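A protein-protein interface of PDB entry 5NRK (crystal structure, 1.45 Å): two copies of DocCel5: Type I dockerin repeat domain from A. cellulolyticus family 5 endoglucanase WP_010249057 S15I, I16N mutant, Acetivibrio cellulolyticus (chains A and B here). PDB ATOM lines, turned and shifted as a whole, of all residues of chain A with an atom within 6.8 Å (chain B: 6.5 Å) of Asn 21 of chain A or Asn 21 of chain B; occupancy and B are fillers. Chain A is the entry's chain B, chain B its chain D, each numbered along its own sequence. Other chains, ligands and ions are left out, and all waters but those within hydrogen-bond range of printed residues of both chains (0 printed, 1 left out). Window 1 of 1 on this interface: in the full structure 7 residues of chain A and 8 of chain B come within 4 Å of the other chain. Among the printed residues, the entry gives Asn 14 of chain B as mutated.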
ATOM      1  N   PHE A  16      -3.654 -12.061 -10.540  1.00  0.00           N
ATOM      2  CA  PHE A  16      -2.958 -12.527  -9.326  1.00  0.00           C
ATOM      3  C   PHE A  16      -1.775 -13.428  -9.682  1.00  0.00           C
ATOM      4  O   PHE A  16      -0.675 -13.278  -9.138  1.00  0.00           O
ATOM      5  CB  PHE A  16      -3.967 -13.225  -8.413  1.00  0.00           C
ATOM      6  CG  PHE A  16      -3.411 -13.643  -7.068  1.00  0.00           C
ATOM      7  CD1 PHE A  16      -3.165 -12.723  -6.058  1.00  0.00           C
ATOM      8  CD2 PHE A  16      -3.177 -14.975  -6.817  1.00  0.00           C
ATOM      9  CE1 PHE A  16      -2.665 -13.148  -4.814  1.00  0.00           C
ATOM     10  CE2 PHE A  16      -2.707 -15.401  -5.577  1.00  0.00           C
ATOM     11  CZ  PHE A  16      -2.440 -14.478  -4.589  1.00  0.00           C
ATOM     12  N   ALA A  17      -2.002 -14.361 -10.600  1.00  0.00           N
ATOM     13  CA  ALA A  17      -0.955 -15.248 -11.076  1.00  0.00           C
ATOM     14  C   ALA A  17       0.186 -14.454 -11.702  1.00  0.00           C
ATOM     15  O   ALA A  17       1.360 -14.750 -11.463  1.00  0.00           O
ATOM     16  CB  ALA A  17      -1.517 -16.257 -12.063  1.00  0.00           C
ATOM     17  N   LEU A  18      -0.144 -13.461 -12.523  1.00  0.00           N
ATOM     18  CA  LEU A  18       0.879 -12.630 -13.146  1.00  0.00           C
ATOM     19  C   LEU A  18       1.689 -11.886 -12.099  1.00  0.00           C
ATOM     20  O   LEU A  18       2.918 -11.801 -12.189  1.00  0.00           O
ATOM     21  CB  LEU A  18       0.238 -11.630 -14.122  1.00  0.00           C
ATOM     22  CG  LEU A  18      -0.270 -12.232 -15.424  1.00  0.00           C
ATOM     23  CD1 LEU A  18      -1.237 -11.280 -16.096  1.00  0.00           C
ATOM     24  CD2 LEU A  18       0.884 -12.573 -16.352  1.00  0.00           C
ATOM     25  N   MET A  19       1.013 -11.299 -11.123  1.00  0.00           N
ATOM     26  CA  MET A  19       1.711 -10.584 -10.052  1.00  0.00           C
ATOM     27  C   MET A  19       2.648 -11.525  -9.284  1.00  0.00           C
ATOM     28  O   MET A  19       3.787 -11.156  -8.982  1.00  0.00           O
ATOM     29  CB  MET A  19       0.722  -9.881  -9.142  1.00  0.00           C
ATOM     30  CG  MET A  19       1.322  -9.307  -7.875  1.00  0.00           C
ATOM     31  SD  MET A  19       2.123  -7.758  -8.243  1.00  0.00           S
ATOM     32  CE  MET A  19       0.702  -6.667  -8.533  1.00  0.00           C
ATOM     33  N   ARG A  20       2.172 -12.736  -8.967  1.00  0.00           N
ATOM     34  CA  ARG A  20       3.009 -13.686  -8.259  1.00  0.00           C
ATOM     35  C   ARG A  20       4.244 -14.011  -9.086  1.00  0.00           C
ATOM     36  O   ARG A  20       5.378 -14.004  -8.596  1.00  0.00           O
ATOM     37  CB  ARG A  20       2.244 -14.979  -7.937  1.00  0.00           C
ATOM     38  CG  ARG A  20       3.026 -15.862  -6.986  1.00  0.00           C
ATOM     39  CD  ARG A  20       2.241 -17.075  -6.506  1.00  0.00           C
ATOM     40  NE  ARG A  20       2.964 -17.695  -5.379  1.00  0.00           N
ATOM     41  CZ  ARG A  20       3.843 -18.661  -5.470  1.00  0.00           C
ATOM     42  NH1 ARG A  20       4.145 -19.210  -6.647  1.00  0.00           N
ATOM     43  NH2 ARG A  20       4.454 -19.085  -4.371  1.00  0.00           N
ATOM     44  N   ASN A  21       4.039 -14.295 -10.364  1.00  0.00           N
ATOM     45  CA  ASN A  21       5.135 -14.597 -11.271  1.00  0.00           C
ATOM     46  C   ASN A  21       6.112 -13.461 -11.436  1.00  0.00           C
ATOM     47  O   ASN A  21       7.333 -13.682 -11.473  1.00  0.00           O
ATOM     48  CB  ASN A  21       4.632 -15.137 -12.606  1.00  0.00           C
ATOM     49  CG  ASN A  21       4.187 -16.589 -12.482  1.00  0.00           C
ATOM     50  OD1 ASN A  21       4.993 -17.438 -12.067  1.00  0.00           O
ATOM     51  ND2 ASN A  21       2.949 -16.915 -12.869  1.00  0.00           N
ATOM     52  N   TYR A  22       5.608 -12.228 -11.481  1.00  0.00           N
ATOM     53  CA  TYR A  22       6.471 -11.063 -11.539  1.00  0.00           C
ATOM     54  C   TYR A  22       7.358 -10.972 -10.294  1.00  0.00           C
ATOM     55  O   TYR A  22       8.577 -10.776 -10.391  1.00  0.00           O
ATOM     56  CB  TYR A  22       5.604  -9.812 -11.652  1.00  0.00           C
ATOM     57  CG  TYR A  22       6.361  -8.532 -11.592  1.00  0.00           C
ATOM     58  CD1 TYR A  22       7.104  -8.098 -12.672  1.00  0.00           C
ATOM     59  CD2 TYR A  22       6.356  -7.759 -10.431  1.00  0.00           C
ATOM     60  CE1 TYR A  22       7.813  -6.909 -12.608  1.00  0.00           C
ATOM     61  CE2 TYR A  22       7.063  -6.573 -10.344  1.00  0.00           C
ATOM     62  CZ  TYR A  22       7.784  -6.157 -11.448  1.00  0.00           C
ATOM     63  OH  TYR A  22       8.491  -4.970 -11.380  1.00  0.00           O
ATOM     64  N   LEU A  23       6.753 -11.151  -9.122  1.00  0.00           N
ATOM     65  CA  LEU A  23       7.508 -11.049  -7.866  1.00  0.00           C
ATOM     66  C   LEU A  23       8.484 -12.202  -7.662  1.00  0.00           C
ATOM     67  O   LEU A  23       9.473 -12.038  -6.951  1.00  0.00           O
ATOM     68  CB  LEU A  23       6.554 -10.902  -6.680  1.00  0.00           C
ATOM     69  CG  LEU A  23       5.719  -9.623  -6.677  1.00  0.00           C
ATOM     70  CD1 LEU A  23       4.706  -9.669  -5.556  1.00  0.00           C
ATOM     71  CD2 LEU A  23       6.574  -8.379  -6.576  1.00  0.00           C
ATOM     72  N   LEU A  24       8.287 -13.310  -8.362  1.00  0.00           N
ATOM     73  CA  LEU A  24       9.232 -14.415  -8.347  1.00  0.00           C
ATOM     74  C   LEU A  24      10.278 -14.370  -9.465  1.00  0.00           C
ATOM     75  O   LEU A  24      11.117 -15.250  -9.571  1.00  0.00           O
ATOM     76  CB  LEU A  24       8.477 -15.749  -8.400  1.00  0.00           C
ATOM     77  CG  LEU A  24       7.759 -16.077  -7.085  1.00  0.00           C
ATOM     78  CD1 LEU A  24       6.830 -17.251  -7.293  1.00  0.00           C
ATOM     79  CD2 LEU A  24       8.744 -16.374  -5.966  1.00  0.00           C
ATOM     80  N   GLY A  25      10.252 -13.330 -10.294  1.00  0.00           N
ATOM     81  CA  GLY A  25      11.197 -13.227 -11.387  1.00  0.00           C
ATOM     82  C   GLY A  25      10.921 -14.065 -12.628  1.00  0.00           C
ATOM     83  O   GLY A  25      11.829 -14.285 -13.428  1.00  0.00           O
ATOM     84  N   ASN A  26       9.671 -14.508 -12.792  1.00  0.00           N
ATOM     85  CA  ASN A  26       9.234 -15.265 -13.964  1.00  0.00           C
ATOM     86  C   ASN A  26       8.573 -14.364 -15.004  1.00  0.00           C
ATOM     87  O   ASN A  26       8.109 -14.878 -16.006  1.00  0.00           O
ATOM     88  CB  ASN A  26       8.271 -16.393 -13.577  1.00  0.00           C
ATOM     89  CG  ASN A  26       8.962 -17.549 -12.902  1.00  0.00           C
ATOM     90  OD1 ASN A  26      10.123 -17.826 -13.171  1.00  0.00           O
ATOM     91  ND2 ASN A  26       8.233 -18.225 -12.015  1.00  0.00           N
ATOM     92  N   LEU A  27       8.518 -13.057 -14.764  1.00  0.00           N
ATOM     93  CA  LEU A  27       8.121 -12.047 -15.768  1.00  0.00           C
ATOM     94  C   LEU A  27       9.050 -10.853 -15.671  1.00  0.00           C
ATOM     95  O   LEU A  27       9.394 -10.443 -14.565  1.00  0.00           O
ATOM     96  CB  LEU A  27       6.714 -11.539 -15.492  1.00  0.00           C
ATOM     97  CG  LEU A  27       5.539 -12.467 -15.691  1.00  0.00           C
ATOM     98  CD1 LEU A  27       4.284 -11.737 -15.248  1.00  0.00           C
ATOM     99  CD2 LEU A  27       5.407 -12.870 -17.156  1.00  0.00           C
ATOM    100  N   LYS A  28       9.436 -10.273 -16.796  1.00  0.00           N
ATOM    101  CA  LYS A  28      10.290  -9.076 -16.741  1.00  0.00           C
ATOM    102  C   LYS A  28       9.433  -7.844 -16.484  1.00  0.00           C
ATOM    103  O   LYS A  28       9.848  -6.894 -15.806  1.00  0.00           O
ATOM    104  CB  LYS A  28      11.076  -8.894 -18.038  1.00  0.00           C
ATOM    105  CG  LYS A  28      12.051 -10.017 -18.361  1.00  0.00           C
ATOM    106  CD  LYS A  28      12.638  -9.847 -19.754  1.00  0.00           C
ATOM    107  CE  LYS A  28      13.770 -10.836 -19.999  1.00  0.00           C
ATOM    108  NZ  LYS A  28      13.307 -12.256 -20.030  1.00  0.00           N
ATOM    109  N   PHE A  30       4.850  -6.549 -17.013  1.00  0.00           N
ATOM    110  CA  PHE A  30       3.453  -6.933 -17.188  1.00  0.00           C
ATOM    111  C   PHE A  30       2.984  -6.624 -18.603  1.00  0.00           C
ATOM    112  O   PHE A  30       3.515  -5.719 -19.248  1.00  0.00           O
ATOM    113  CB  PHE A  30       2.578  -6.171 -16.197  1.00  0.00           C
ATOM    114  CG  PHE A  30       2.780  -6.574 -14.772  1.00  0.00           C
ATOM    115  CD1 PHE A  30       2.348  -7.794 -14.328  1.00  0.00           C
ATOM    116  CD2 PHE A  30       3.379  -5.723 -13.873  1.00  0.00           C
ATOM    117  CE1 PHE A  30       2.505  -8.177 -13.025  1.00  0.00           C
ATOM    118  CE2 PHE A  30       3.566  -6.113 -12.562  1.00  0.00           C
ATOM    119  CZ  PHE A  30       3.101  -7.338 -12.133  1.00  0.00           C
ATOM    120  N   PHE A  52       0.569  -7.230  -3.967  1.00  0.00           N
ATOM    121  CA  PHE A  52       0.106  -8.608  -4.068  1.00  0.00           C
ATOM    122  C   PHE A  52      -0.963  -8.916  -3.005  1.00  0.00           C
ATOM    123  O   PHE A  52      -1.994  -9.518  -3.301  1.00  0.00           O
ATOM    124  CB  PHE A  52       1.353  -9.498  -3.979  1.00  0.00           C
ATOM    125  CG  PHE A  52       1.145 -10.965  -4.239  1.00  0.00           C
ATOM    126  CD1 PHE A  52       0.508 -11.431  -5.386  1.00  0.00           C
ATOM    127  CD2 PHE A  52       1.666 -11.888  -3.356  1.00  0.00           C
ATOM    128  CE1 PHE A  52       0.412 -12.793  -5.618  1.00  0.00           C
ATOM    129  CE2 PHE A  52       1.555 -13.250  -3.586  1.00  0.00           C
ATOM    130  CZ  PHE A  52       0.890 -13.694  -4.698  1.00  0.00           C
ATOM    131  N   ASN B  14      -0.645 -22.080  -6.617  1.00  0.00           N
ATOM    132  CA  ASN B  14       0.672 -21.596  -7.042  1.00  0.00           C
ATOM    133  C   ASN B  14       1.324 -22.489  -8.093  1.00  0.00           C
ATOM    134  O   ASN B  14       2.032 -21.988  -8.979  1.00  0.00           O
ATOM    135  CB  ASN B  14       1.553 -21.417  -5.826  1.00  0.00           C
ATOM    136  CG  ASN B  14       0.992 -20.397  -4.863  1.00  0.00           C
ATOM    137  OD1 ASN B  14       0.184 -19.551  -5.249  1.00  0.00           O
ATOM    138  ND2 ASN B  14       1.401 -20.487  -3.619  1.00  0.00           N
ATOM    139  N   PHE B  16      -0.552 -24.043 -10.295  1.00  0.00           N
ATOM    140  CA  PHE B  16      -1.343 -23.643 -11.466  1.00  0.00           C
ATOM    141  C   PHE B  16      -0.795 -22.357 -12.099  1.00  0.00           C
ATOM    142  O   PHE B  16      -0.625 -22.258 -13.320  1.00  0.00           O
ATOM    143  CB  PHE B  16      -2.821 -23.518 -11.038  1.00  0.00           C
ATOM    144  CG  PHE B  16      -3.775 -23.164 -12.137  1.00  0.00           C
ATOM    145  CD1 PHE B  16      -4.234 -24.133 -13.008  1.00  0.00           C
ATOM    146  CD2 PHE B  16      -4.277 -21.876 -12.243  1.00  0.00           C
ATOM    147  CE1 PHE B  16      -5.151 -23.820 -13.996  1.00  0.00           C
ATOM    148  CE2 PHE B  16      -5.202 -21.549 -13.239  1.00  0.00           C
ATOM    149  CZ  PHE B  16      -5.628 -22.529 -14.113  1.00  0.00           C
ATOM    150  N   ALA B  17      -0.461 -21.394 -11.256  1.00  0.00           N
ATOM    151  CA  ALA B  17       0.111 -20.132 -11.723  1.00  0.00           C
ATOM    152  C   ALA B  17       1.429 -20.342 -12.440  1.00  0.00           C
ATOM    153  O   ALA B  17       1.701 -19.673 -13.446  1.00  0.00           O
ATOM    154  CB  ALA B  17       0.253 -19.154 -10.568  1.00  0.00           C
ATOM    155  N   LEU B  18       2.288 -21.224 -11.914  1.00  0.00           N
ATOM    156  CA  LEU B  18       3.541 -21.508 -12.600  1.00  0.00           C
ATOM    157  C   LEU B  18       3.316 -22.164 -13.951  1.00  0.00           C
ATOM    158  O   LEU B  18       3.976 -21.832 -14.946  1.00  0.00           O
ATOM    159  CB  LEU B  18       4.426 -22.391 -11.727  1.00  0.00           C
ATOM    160  CG  LEU B  18       4.976 -21.690 -10.486  1.00  0.00           C
ATOM    161  CD1 LEU B  18       5.549 -22.707  -9.512  1.00  0.00           C
ATOM    162  CD2 LEU B  18       6.019 -20.655 -10.831  1.00  0.00           C
ATOM    163  N   MET B  19       2.400 -23.101 -13.985  1.00  0.00           N
ATOM    164  CA  MET B  19       2.152 -23.751 -15.257  1.00  0.00           C
ATOM    165  C   MET B  19       1.574 -22.774 -16.276  1.00  0.00           C
ATOM    166  O   MET B  19       1.920 -22.864 -17.385  1.00  0.00           O
ATOM    167  CB  MET B  19       1.231 -24.977 -15.118  1.00  0.00           C
ATOM    168  CG  MET B  19       1.360 -25.962 -16.327  1.00  0.00           C
ATOM    169  SD  MET B  19       0.369 -27.464 -16.061  1.00  0.00           S
ATOM    170  CE  MET B  19       0.109 -27.427 -14.230  1.00  0.00           C
ATOM    171  N   ARG B  20       0.704 -21.858 -15.874  1.00  0.00           N
ATOM    172  CA  ARG B  20       0.224 -20.853 -16.808  1.00  0.00           C
ATOM    173  C   ARG B  20       1.381 -20.045 -17.418  1.00  0.00           C
ATOM    174  O   ARG B  20       1.467 -19.820 -18.628  1.00  0.00           O
ATOM    175  CB  ARG B  20      -0.779 -19.912 -16.121  1.00  0.00           C
ATOM    176  CG  ARG B  20      -1.489 -19.012 -17.116  1.00  0.00           C
ATOM    177  CD  ARG B  20      -2.590 -18.180 -16.464  1.00  0.00           C
ATOM    178  NE  ARG B  20      -3.377 -17.431 -17.456  1.00  0.00           N
ATOM    179  CZ  ARG B  20      -3.094 -16.211 -17.918  1.00  0.00           C
ATOM    180  NH1 ARG B  20      -2.071 -15.507 -17.472  1.00  0.00           N
ATOM    181  NH2 ARG B  20      -3.881 -15.689 -18.863  1.00  0.00           N
ATOM    182  N   ASN B  21       2.276 -19.597 -16.550  1.00  0.00           N
ATOM    183  CA  ASN B  21       3.437 -18.830 -16.949  1.00  0.00           C
ATOM    184  C   ASN B  21       4.356 -19.587 -17.914  1.00  0.00           C
ATOM    185  O   ASN B  21       4.855 -19.017 -18.904  1.00  0.00           O
ATOM    186  CB  ASN B  21       4.167 -18.381 -15.668  1.00  0.00           C
ATOM    187  CG  ASN B  21       5.458 -17.619 -15.938  1.00  0.00           C
ATOM    188  OD1 ASN B  21       6.562 -18.197 -16.031  1.00  0.00           O
ATOM    189  ND2 ASN B  21       5.341 -16.314 -16.019  1.00  0.00           N
ATOM    190  N   TYR B  22       4.550 -20.878 -17.625  1.00  0.00           N
ATOM    191  CA  TYR B  22       5.303 -21.764 -18.525  1.00  0.00           C
ATOM    192  C   TYR B  22       4.651 -21.831 -19.902  1.00  0.00           C
ATOM    193  O   TYR B  22       5.317 -21.696 -20.930  1.00  0.00           O
ATOM    194  CB  TYR B  22       5.410 -23.153 -17.900  1.00  0.00           C
ATOM    195  CG  TYR B  22       6.033 -24.187 -18.802  1.00  0.00           C
ATOM    196  CD1 TYR B  22       7.386 -24.170 -19.065  1.00  0.00           C
ATOM    197  CD2 TYR B  22       5.262 -25.158 -19.411  1.00  0.00           C
ATOM    198  CE1 TYR B  22       7.964 -25.117 -19.895  1.00  0.00           C
ATOM    199  CE2 TYR B  22       5.813 -26.106 -20.253  1.00  0.00           C
ATOM    200  CZ  TYR B  22       7.165 -26.077 -20.504  1.00  0.00           C
ATOM    201  OH  TYR B  22       7.749 -27.022 -21.340  1.00  0.00           O
ATOM    202  N   LEU B  23       3.350 -22.075 -19.917  1.00  0.00           N
ATOM    203  CA  LEU B  23       2.648 -22.252 -21.184  1.00  0.00           C
ATOM    204  C   LEU B  23       2.566 -20.973 -22.007  1.00  0.00           C
ATOM    205  O   LEU B  23       2.414 -21.040 -23.227  1.00  0.00           O
ATOM    206  CB  LEU B  23       1.270 -22.873 -20.959  1.00  0.00           C
ATOM    207  CG  LEU B  23       1.310 -24.289 -20.407  1.00  0.00           C
ATOM    208  CD1 LEU B  23      -0.076 -24.773 -20.079  1.00  0.00           C
ATOM    209  CD2 LEU B  23       1.993 -25.267 -21.351  1.00  0.00           C
ATOM    210  N   LEU B  24       2.723 -19.824 -21.361  1.00  0.00           N
ATOM    211  CA  LEU B  24       2.802 -18.550 -22.073  1.00  0.00           C
ATOM    212  C   LEU B  24       4.229 -18.166 -22.501  1.00  0.00           C
ATOM    213  O   LEU B  24       4.445 -17.093 -23.045  1.00  0.00           O
ATOM    214  CB  LEU B  24       2.141 -17.457 -21.228  1.00  0.00           C
ATOM    215  CG  LEU B  24       0.610 -17.591 -21.196  1.00  0.00           C
ATOM    216  CD1 LEU B  24       0.020 -16.705 -20.108  1.00  0.00           C
ATOM    217  CD2 LEU B  24      -0.009 -17.253 -22.543  1.00  0.00           C
ATOM    218  N   GLY B  25       5.171 -19.042 -22.250  1.00  0.00           N
ATOM    219  CA  GLY B  25       6.531 -18.850 -22.730  1.00  0.00           C
ATOM    220  C   GLY B  25       7.526 -18.154 -21.802  1.00  0.00           C
ATOM    221  O   GLY B  25       8.471 -17.646 -22.367  1.00  0.00           O
ATOM    222  N   ASN B  26       7.222 -18.066 -20.573  1.00  0.00           N
ATOM    223  CA  ASN B  26       8.064 -17.358 -19.640  1.00  0.00           C
ATOM    224  C   ASN B  26       9.083 -18.304 -18.946  1.00  0.00           C
ATOM    225  O   ASN B  26      10.083 -18.519 -19.572  1.00  0.00           O
ATOM    226  CB  ASN B  26       7.190 -16.561 -18.707  1.00  0.00           C
ATOM    227  CG  ASN B  26       6.325 -15.577 -19.428  1.00  0.00           C
ATOM    228  OD1 ASN B  26       6.800 -14.581 -19.870  1.00  0.00           O
ATOM    229  ND2 ASN B  26       5.046 -15.876 -19.513  1.00  0.00           N
ATOM    230  N   LEU B  27       8.835 -18.865 -17.745  1.00  0.00           N
ATOM    231  CA  LEU B  27       9.777 -19.723 -17.057  1.00  0.00           C
ATOM    232  C   LEU B  27      10.006 -20.989 -17.855  1.00  0.00           C
ATOM    233  O   LEU B  27       9.068 -21.636 -18.323  1.00  0.00           O
ATOM    234  CB  LEU B  27       9.264 -20.069 -15.657  1.00  0.00           C
ATOM    235  CG  LEU B  27       8.202 -21.169 -15.576  1.00  0.00           C
ATOM    236  CD1 LEU B  27       8.854 -22.531 -15.402  1.00  0.00           C
ATOM    237  CD2 LEU B  27       7.224 -20.889 -14.445  1.00  0.00           C
ATOM    238  N   LYS B  28      11.275 -21.324 -18.002  1.00  0.00           N
ATOM    239  CA  LYS B  28      11.714 -22.481 -18.770  1.00  0.00           C
ATOM    240  C   LYS B  28      11.972 -23.702 -17.886  1.00  0.00           C
ATOM    241  O   LYS B  28      11.827 -24.837 -18.353  1.00  0.00           O
ATOM    242  CB  LYS B  28      12.966 -22.105 -19.564  1.00  0.00           C
ATOM    243  CG  LYS B  28      12.718 -20.999 -20.583  1.00  0.00           C
ATOM    244  CD  LYS B  28      11.627 -21.380 -21.563  1.00  0.00           C
ATOM    245  CE  LYS B  28      11.316 -20.259 -22.539  1.00  0.00           C
ATOM    246  NZ  LYS B  28      10.255 -20.729 -23.474  1.00  0.00           N
ATOM    247  N   PHE B  52      -2.461 -28.614 -17.737  1.00  0.00           N
ATOM    248  CA  PHE B  52      -3.006 -27.411 -17.103  1.00  0.00           C
ATOM    249  C   PHE B  52      -4.480 -27.615 -16.760  1.00  0.00           C
ATOM    250  O   PHE B  52      -4.938 -27.289 -15.661  1.00  0.00           O
ATOM    251  CB  PHE B  52      -2.780 -26.254 -18.088  1.00  0.00           C
ATOM    252  CG  PHE B  52      -3.128 -24.873 -17.598  1.00  0.00           C
ATOM    253  CD1 PHE B  52      -2.585 -24.340 -16.444  1.00  0.00           C
ATOM    254  CD2 PHE B  52      -3.892 -24.049 -18.402  1.00  0.00           C
ATOM    255  CE1 PHE B  52      -2.853 -23.032 -16.079  1.00  0.00           C
ATOM    256  CE2 PHE B  52      -4.174 -22.758 -18.025  1.00  0.00           C
ATOM    257  CZ  PHE B  52      -3.653 -22.245 -16.871  1.00  0.00           C
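Among the printed residues, pairs that only touch across the chains: Asn 26 of chain A with Asn 26 of chain B, Asn 21 of chain A with Asn 21 of chain B, Asn 26 of chain A with Leu 27 of chain B, Asn 26 of chain A with Leu 18 of chain B, Leu 27 of chain A with Asn 26 of chain B, Asn 21 of chain A with Leu 18 of chain B, Leu 27 of chain A with Asn 21 of chain B and Ala 17 of chain A with Ala 17 of chain B.
ND2 of Asn 21 of chain B sits at hydrogen-bond distance from O of Asn 26 of chain A, at 3.1 Å.
O of Ala 17 of chain B sits at hydrogen-bond distance from ND2 of Asn 21 of chain A (3.1 Å).
The side-chain amide oxygen (OD1) of Asn 14 of chain B is in hydrogen-bond range of the guanidinium group (NE) of Arg 20 of chain A, at 3.3 Å.
Asn 21 of chain A touches just these residues of chain B: Ala 17, Leu 18 and Asn 21.
Of the printed residues of chain B, Asn 26 of chain A touches Leu 18, Asn 21, Asn 26 and Leu 27.
Of the printed residues of chain B, Leu 27 of chain A touches Asn 21 and Asn 26.
Printed residues of chain A within 4 Å of Asn 14 of chain B: Arg 20.
Phe 16 of chain B touches none of the printed residues of chain A.
Printed residues of chain A within 4 Å of Ala 17 of chain B: Ala 17 (3.7 Å) and Asn 21 (3.1 Å).
Asn 21 of chain B touches just these residues of chain A: Asn 21, Asn 26 and Leu 27.
Printed residues of chain A within 4 Å of Asn 26 of chain B: Asn 26 (3.3 Å) and Leu 27 (3.5 Å).
The nearest residue of chain A that does not touch Asn 21 of chain B is Leu 18 of chain A (5.8 Å).
Ala 17 of chain A touches its own counterpart, Ala 17 of chain B.
Asn 21 of chain A touches Ala 17 of chain B, but with the chains exchanged Ala 17 of chain A does not touch Asn 21 of chain B (6.2 Å).
Asn 21 of chain A touches Leu 18 of chain B, but with the chains exchanged Leu 18 of chain A does not touch Asn 21 of chain B (5.8 Å).
Asn 26 of chain A touches Asn 21 of chain B, but with the chains exchanged Asn 21 of chain A does not touch Asn 26 of chain B (6.8 Å).
Of the 11 pairs that touch across the chains among the printed residues, 5 have their exchanged pair printed and touching as well.
Of the 15 printed residues of chain A, 5 touch a printed residue of chain B.
Printed residues of chain A that touch a printed residue of chain B: Ala 17, Arg 20, Asn 21, Asn 26 and Leu 27.
Hydrophobic or aromatic side chains of chain A that line the printed part of chain B: Ala 17 and Leu 27.
Printed residues of chain B that touch a printed residue of chain A: Asn 14, Ala 17, Leu 18, Asn 21, Asn 26 and Leu 27.
Among the printed residues, no Asp or Glu carboxylate lies within 4 Å of a Lys or Arg side-chain nitrogen of the other chain.
N of Asn 26 of chain A lies within hydrogen-bond range of O of Asn 21 of chain A, at 2.8 Å.
The side-chain amide nitrogen (ND2) of Asn 21 of chain A sits at hydrogen-bond distance from the backbone carbonyl oxygen (O) of Ala 17 of chain A.
The backbone carbonyl oxygen (O) of Asn 21 of chain B sits at hydrogen-bond distance from the backbone NH (N) of Asn 26 of chain B, at 3.0 Å.
The side-chain amide oxygen (OD1) of Asn 21 of chain B sits at hydrogen-bond distance from the backbone NH (N) of Leu 27 of chain B, 2.9 Å away.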
